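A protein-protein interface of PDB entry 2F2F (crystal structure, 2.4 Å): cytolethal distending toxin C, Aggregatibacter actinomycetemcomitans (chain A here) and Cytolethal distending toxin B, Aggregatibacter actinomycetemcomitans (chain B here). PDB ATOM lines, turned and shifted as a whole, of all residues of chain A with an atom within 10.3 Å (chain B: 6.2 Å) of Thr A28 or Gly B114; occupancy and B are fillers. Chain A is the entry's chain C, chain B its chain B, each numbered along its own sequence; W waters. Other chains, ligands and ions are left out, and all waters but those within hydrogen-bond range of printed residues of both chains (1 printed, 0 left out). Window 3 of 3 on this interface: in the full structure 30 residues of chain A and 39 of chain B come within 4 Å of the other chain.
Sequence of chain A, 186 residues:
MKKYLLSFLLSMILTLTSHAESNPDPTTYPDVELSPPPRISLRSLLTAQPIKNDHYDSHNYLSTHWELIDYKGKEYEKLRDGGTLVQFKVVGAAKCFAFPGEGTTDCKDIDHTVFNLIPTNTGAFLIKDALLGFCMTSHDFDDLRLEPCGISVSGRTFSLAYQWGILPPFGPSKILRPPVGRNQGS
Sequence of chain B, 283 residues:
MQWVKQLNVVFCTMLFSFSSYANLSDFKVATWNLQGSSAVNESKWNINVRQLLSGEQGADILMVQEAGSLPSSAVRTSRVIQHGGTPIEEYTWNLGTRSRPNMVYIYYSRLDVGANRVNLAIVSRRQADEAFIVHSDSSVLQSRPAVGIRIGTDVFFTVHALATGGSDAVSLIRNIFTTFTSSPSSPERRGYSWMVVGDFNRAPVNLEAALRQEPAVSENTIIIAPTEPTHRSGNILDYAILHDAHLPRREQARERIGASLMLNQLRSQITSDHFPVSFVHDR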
ATOM      1  N   ASP A  25     -28.011  25.193 -10.309  1.00  0.00           N
ATOM      2  CA  ASP A  25     -27.520  25.706 -11.632  1.00  0.00           C
ATOM      3  C   ASP A  25     -25.981  25.906 -11.596  1.00  0.00           C
ATOM      4  O   ASP A  25     -25.284  24.930 -11.350  1.00  0.00           O
ATOM      5  CB  ASP A  25     -28.283  26.988 -11.976  1.00  0.00           C
ATOM      6  CG  ASP A  25     -28.512  27.139 -13.468  1.00  0.00           C
ATOM      7  OD1 ASP A  25     -27.946  26.327 -14.236  1.00  0.00           O
ATOM      8  OD2 ASP A  25     -29.249  28.069 -13.874  1.00  0.00           O
ATOM      9  N   PRO A  26     -25.421  27.112 -11.873  1.00  0.00           N
ATOM     10  CA  PRO A  26     -23.956  27.229 -11.817  1.00  0.00           C
ATOM     11  C   PRO A  26     -23.485  27.501 -10.388  1.00  0.00           C
ATOM     12  O   PRO A  26     -22.587  28.301 -10.161  1.00  0.00           O
ATOM     13  CB  PRO A  26     -23.641  28.396 -12.738  1.00  0.00           C
ATOM     14  CG  PRO A  26     -24.792  29.281 -12.577  1.00  0.00           C
ATOM     15  CD  PRO A  26     -26.000  28.406 -12.303  1.00  0.00           C
ATOM     16  N   THR A  27     -24.154  26.885  -9.431  1.00  0.00           N
ATOM     17  CA  THR A  27     -23.826  27.104  -8.033  1.00  0.00           C
ATOM     18  C   THR A  27     -22.369  26.824  -7.649  1.00  0.00           C
ATOM     19  O   THR A  27     -21.712  25.972  -8.232  1.00  0.00           O
ATOM     20  CB  THR A  27     -24.753  26.252  -7.124  1.00  0.00           C
ATOM     21  OG1 THR A  27     -24.494  26.567  -5.751  1.00  0.00           O
ATOM     22  CG2 THR A  27     -24.520  24.767  -7.344  1.00  0.00           C
ATOM     23  N   THR A  28     -21.886  27.581  -6.662  1.00  0.00           N
ATOM     24  CA  THR A  28     -20.536  27.453  -6.108  1.00  0.00           C
ATOM     25  C   THR A  28     -20.457  26.128  -5.326  1.00  0.00           C
ATOM     26  O   THR A  28     -19.367  25.600  -5.080  1.00  0.00           O
ATOM     27  CB  THR A  28     -20.235  28.618  -5.122  1.00  0.00           C
ATOM     28  OG1 THR A  28     -20.302  29.871  -5.804  1.00  0.00           O
ATOM     29  CG2 THR A  28     -18.880  28.475  -4.516  1.00  0.00           C
ATOM     30  N   TYR A  29     -21.618  25.586  -4.960  1.00  0.00           N
ATOM     31  CA  TYR A  29     -21.684  24.347  -4.190  1.00  0.00           C
ATOM     32  C   TYR A  29     -22.519  23.292  -4.869  1.00  0.00           C
ATOM     33  O   TYR A  29     -23.685  23.101  -4.525  1.00  0.00           O
ATOM     34  CB  TYR A  29     -22.276  24.635  -2.819  1.00  0.00           C
ATOM     35  CG  TYR A  29     -21.499  25.696  -2.095  1.00  0.00           C
ATOM     36  CD1 TYR A  29     -20.277  25.388  -1.510  1.00  0.00           C
ATOM     37  CD2 TYR A  29     -21.949  27.006  -2.038  1.00  0.00           C
ATOM     38  CE1 TYR A  29     -19.521  26.345  -0.891  1.00  0.00           C
ATOM     39  CE2 TYR A  29     -21.190  27.984  -1.417  1.00  0.00           C
ATOM     40  CZ  TYR A  29     -19.971  27.639  -0.845  1.00  0.00           C
ATOM     41  OH  TYR A  29     -19.177  28.580  -0.233  1.00  0.00           O
ATOM     42  N   PRO A  30     -21.907  22.549  -5.802  1.00  0.00           N
ATOM     43  CA  PRO A  30     -22.620  21.498  -6.531  1.00  0.00           C
ATOM     44  C   PRO A  30     -23.041  20.327  -5.666  1.00  0.00           C
ATOM     45  O   PRO A  30     -23.807  19.467  -6.099  1.00  0.00           O
ATOM     46  CB  PRO A  30     -21.623  21.075  -7.613  1.00  0.00           C
ATOM     47  CG  PRO A  30     -20.272  21.421  -7.041  1.00  0.00           C
ATOM     48  CD  PRO A  30     -20.498  22.664  -6.221  1.00  0.00           C
ATOM     49  N   ASP A  31     -22.546  20.282  -4.440  1.00  0.00           N
ATOM     50  CA  ASP A  31     -22.916  19.182  -3.570  1.00  0.00           C
ATOM     51  C   ASP A  31     -24.379  19.349  -3.170  1.00  0.00           C
ATOM     52  O   ASP A  31     -25.060  18.375  -2.847  1.00  0.00           O
ATOM     53  CB  ASP A  31     -21.988  19.109  -2.331  1.00  0.00           C
ATOM     54  CG  ASP A  31     -22.246  20.211  -1.303  1.00  0.00           C
ATOM     55  OD1 ASP A  31     -21.913  21.382  -1.570  1.00  0.00           O
ATOM     56  OD2 ASP A  31     -22.766  19.899  -0.216  1.00  0.00           O
ATOM     57  N   VAL A  32     -24.850  20.595  -3.219  1.00  0.00           N
ATOM     58  CA  VAL A  32     -26.221  20.956  -2.875  1.00  0.00           C
ATOM     59  C   VAL A  32     -27.100  20.952  -4.134  1.00  0.00           C
ATOM     60  O   VAL A  32     -27.086  21.893  -4.943  1.00  0.00           O
ATOM     61  CB  VAL A  32     -26.249  22.362  -2.199  1.00  0.00           C
ATOM     62  CG1 VAL A  32     -27.691  22.755  -1.845  1.00  0.00           C
ATOM     63  CG2 VAL A  32     -25.391  22.346  -0.945  1.00  0.00           C
ATOM     64  N   GLU A  33     -27.864  19.877  -4.294  1.00  0.00           N
ATOM     65  CA  GLU A  33     -28.760  19.726  -5.440  1.00  0.00           C
ATOM     66  C   GLU A  33     -29.888  20.752  -5.477  1.00  0.00           C
ATOM     67  O   GLU A  33     -30.450  21.108  -4.443  1.00  0.00           O
ATOM     68  CB  GLU A  33     -29.357  18.320  -5.455  1.00  0.00           C
ATOM     69  CG  GLU A  33     -30.013  17.965  -6.788  1.00  0.00           C
ATOM     70  CD  GLU A  33     -30.668  16.588  -6.782  1.00  0.00           C
ATOM     71  OE1 GLU A  33     -31.552  16.346  -7.642  1.00  0.00           O
ATOM     72  OE2 GLU A  33     -30.298  15.755  -5.919  1.00  0.00           O
ATOM     73  N   ARG B 110     -23.381  36.018   1.501  1.00  0.00           N
ATOM     74  CA  ARG B 110     -23.634  35.531   0.142  1.00  0.00           C
ATOM     75  C   ARG B 110     -22.449  34.710  -0.372  1.00  0.00           C
ATOM     76  O   ARG B 110     -21.583  35.212  -1.082  1.00  0.00           O
ATOM     77  CB  ARG B 110     -23.893  36.717  -0.778  1.00  0.00           C
ATOM     78  CG  ARG B 110     -24.488  36.364  -2.123  1.00  0.00           C
ATOM     79  CD  ARG B 110     -24.658  37.619  -2.942  1.00  0.00           C
ATOM     80  NE  ARG B 110     -24.341  37.400  -4.351  1.00  0.00           N
ATOM     81  CZ  ARG B 110     -23.117  37.184  -4.847  1.00  0.00           C
ATOM     82  NH1 ARG B 110     -22.045  37.155  -4.054  1.00  0.00           N
ATOM     83  NH2 ARG B 110     -22.962  37.002  -6.154  1.00  0.00           N
ATOM     84  N   LEU B 111     -22.456  33.435  -0.016  1.00  0.00           N
ATOM     85  CA  LEU B 111     -21.411  32.482  -0.362  1.00  0.00           C
ATOM     86  C   LEU B 111     -21.519  31.970  -1.790  1.00  0.00           C
ATOM     87  O   LEU B 111     -20.505  31.687  -2.430  1.00  0.00           O
ATOM     88  CB  LEU B 111     -21.448  31.291   0.601  1.00  0.00           C
ATOM     89  CG  LEU B 111     -21.242  31.577   2.100  1.00  0.00           C
ATOM     90  CD1 LEU B 111     -21.560  30.331   2.910  1.00  0.00           C
ATOM     91  CD2 LEU B 111     -19.806  32.025   2.340  1.00  0.00           C
ATOM     92  N   ASP B 112     -22.744  31.847  -2.288  1.00  0.00           N
ATOM     93  CA  ASP B 112     -22.943  31.326  -3.624  1.00  0.00           C
ATOM     94  C   ASP B 112     -22.811  32.421  -4.666  1.00  0.00           C
ATOM     95  O   ASP B 112     -23.801  33.031  -5.072  1.00  0.00           O
ATOM     96  CB  ASP B 112     -24.318  30.673  -3.732  1.00  0.00           C
ATOM     97  CG  ASP B 112     -24.424  29.739  -4.911  1.00  0.00           C
ATOM     98  OD1 ASP B 112     -23.799  30.037  -5.947  1.00  0.00           O
ATOM     99  OD2 ASP B 112     -25.116  28.710  -4.807  1.00  0.00           O
ATOM    100  N   VAL B 113     -21.577  32.635  -5.113  1.00  0.00           N
ATOM    101  CA  VAL B 113     -21.279  33.644  -6.122  1.00  0.00           C
ATOM    102  C   VAL B 113     -21.636  33.096  -7.504  1.00  0.00           C
ATOM    103  O   VAL B 113     -21.914  33.848  -8.437  1.00  0.00           O
ATOM    104  CB  VAL B 113     -19.772  34.072  -6.082  1.00  0.00           C
ATOM    105  CG1 VAL B 113     -19.445  34.697  -4.728  1.00  0.00           C
ATOM    106  CG2 VAL B 113     -18.865  32.873  -6.333  1.00  0.00           C
ATOM    107  N   GLY B 114     -21.636  31.776  -7.622  1.00  0.00           N
ATOM    108  CA  GLY B 114     -21.977  31.142  -8.882  1.00  0.00           C
ATOM    109  C   GLY B 114     -23.459  31.226  -9.204  1.00  0.00           C
ATOM    110  O   GLY B 114     -23.832  31.733 -10.254  1.00  0.00           O
ATOM    111  N   ALA B 115     -24.313  30.764  -8.289  1.00  0.00           N
ATOM    112  CA  ALA B 115     -25.760  30.787  -8.512  1.00  0.00           C
ATOM    113  C   ALA B 115     -26.535  31.609  -7.496  1.00  0.00           C
ATOM    114  O   ALA B 115     -27.737  31.778  -7.646  1.00  0.00           O
ATOM    115  CB  ALA B 115     -26.313  29.381  -8.521  1.00  0.00           C
ATOM    116  N   ASN B 116     -25.871  32.112  -6.466  1.00  0.00           N
ATOM    117  CA  ASN B 116     -26.553  32.919  -5.457  1.00  0.00           C
ATOM    118  C   ASN B 116     -27.747  32.242  -4.789  1.00  0.00           C
ATOM    119  O   ASN B 116     -28.746  32.899  -4.495  1.00  0.00           O
ATOM    120  CB  ASN B 116     -27.033  34.223  -6.090  1.00  0.00           C
ATOM    121  CG  ASN B 116     -27.499  35.234  -5.058  1.00  0.00           C
ATOM    122  OD1 ASN B 116     -26.893  35.386  -3.997  1.00  0.00           O
ATOM    123  ND2 ASN B 116     -28.579  35.930  -5.367  1.00  0.00           N
ATOM    124  N   VAL B 118     -27.114  29.074  -2.525  1.00  0.00           N
ATOM    125  CA  VAL B 118     -26.649  28.430  -1.303  1.00  0.00           C
ATOM    126  C   VAL B 118     -25.946  29.491  -0.458  1.00  0.00           C
ATOM    127  O   VAL B 118     -24.721  29.482  -0.322  1.00  0.00           O
ATOM    128  CB  VAL B 118     -25.655  27.320  -1.602  1.00  0.00           C
ATOM    129  CG1 VAL B 118     -25.286  26.596  -0.331  1.00  0.00           C
ATOM    130  CG2 VAL B 118     -26.246  26.353  -2.605  1.00  0.00           C
ATOM    131  N   GLN B 142     -13.939  23.746  -0.701  1.00  0.00           N
ATOM    132  CA  GLN B 142     -15.271  23.626  -1.283  1.00  0.00           C
ATOM    133  C   GLN B 142     -16.478  23.751  -0.353  1.00  0.00           C
ATOM    134  O   GLN B 142     -17.608  23.938  -0.811  1.00  0.00           O
ATOM    135  CB  GLN B 142     -15.398  22.341  -2.124  1.00  0.00           C
ATOM    136  CG  GLN B 142     -15.262  20.926  -1.523  1.00  0.00           C
ATOM    137  CD  GLN B 142     -15.026  20.827  -0.037  1.00  0.00           C
ATOM    138  OE1 GLN B 142     -14.929  21.823   0.654  1.00  0.00           O
ATOM    139  NE2 GLN B 142     -14.920  19.606   0.463  1.00  0.00           N
HETATM  140  O   HOH W   1     -18.472  23.622  -3.416  1.00  0.00           O
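The side-chain hydroxyl (OG1) of Thr A28 is in hydrogen-bond range of the backbone NH (N) of Gly B114 (3.0 Å). OD2 of Asp B112 is in hydrogen-bond range of OG1 of Thr A27 (2.4 Å). The backbone NH of Val B113 lies within hydrogen-bond range of the side-chain hydroxyl of Thr A28. The backbone NH of Thr A28 lies within hydrogen-bond range of the side-chain carboxylate of Asp B112.
The side-chain carboxylate (OD2) of Asp B112 lies within hydrogen-bond range of the backbone NH (N) of Val B118 (3.1 Å). The side-chain hydroxyl (OG1) of Thr A27 lies close to the backbone NH (N) of Tyr A29. The side-chain carboxylate of Asp B112 sits at hydrogen-bond distance from the backbone NH of Asn B116 (3.0 Å). OD1 of Asp B112 is in hydrogen-bond range of N of Ala B115 (2.5 Å). N of Gly B114 lies within hydrogen-bond range of OD1 of Asp B112 (3.2 Å).
Among the printed residues, pairs that only touch across the chains: Pro A26 with Gly B114 (3.2 Å), Pro A26 with Ala B115 (3.5 Å), Thr A27 with Ala B115 (3.4 Å), Thr A27 with Val B118 (3.6 Å), Thr A28 with Leu B111 (3.8 Å), Tyr A29 with Leu B111 (3.6 Å), Tyr A29 with Val B118 (3.7 Å), Tyr A29 with Gln B142 (3.1 Å) and Val A32 with Val B118 (3.95 Å).
Of the printed residues of chain B, Pro A26 touches Gly B114 (3.2 Å) and Ala B115 (3.5 Å). Printed residues of chain B within 4 Å of Thr A27: Asp B112 (2.4 Å), Ala B115 (3.4 Å) and Val B118 (3.6 Å). Thr A28 touches just these residues of chain B: Leu B111, Asp B112, Val B113 and Gly B114. Of the printed residues of chain B, Tyr A29 touches Leu B111, Val B118 and Gln B142. Asp B112 touches just these residues of chain A: Thr A27 and Thr A28. Of chain A, only Thr A28 (3.1 Å) comes within 4 Å of Val B113. Gly B114 touches just these residues of chain A: Pro A26 (3.2 Å) and Thr A28 (3.0 Å). Of the printed residues of chain A, Val B118 touches Thr A27 (3.6 Å), Tyr A29 (3.7 Å) and Val A32 (3.95 Å). Printed residues of chain A within 4 Å of Gln B142: Tyr A29. The nearest printed residue of chain A that does not touch Gln B142 is Thr A28 (4.9 Å).
Hydrophobic or aromatic side chains of chain A that line the printed part of chain B: Pro A26, Tyr A29 and Val A32. Of the 9 printed residues of chain B, 7 touch a printed residue of chain A. Printed residues of chain B that touch a printed residue of chain A: Leu B111, Asp B112, Val B113, Gly B114, Ala B115, Val B118 and Gln B142. Along chain B the printed residues that touch a printed residue of chain A span positions 111 to 142. Among the printed residues, 13 pairs touch across the chains. Among the printed residues, no Asp or Glu carboxylate lies within 4 Å of a Lys or Arg side-chain nitrogen of the other chain.
Water W1 bridges the backbone carbonyl oxygen of Thr A28 (2.7 Å) and the backbone carbonyl oxygen of Gln B142 (2.8 Å).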
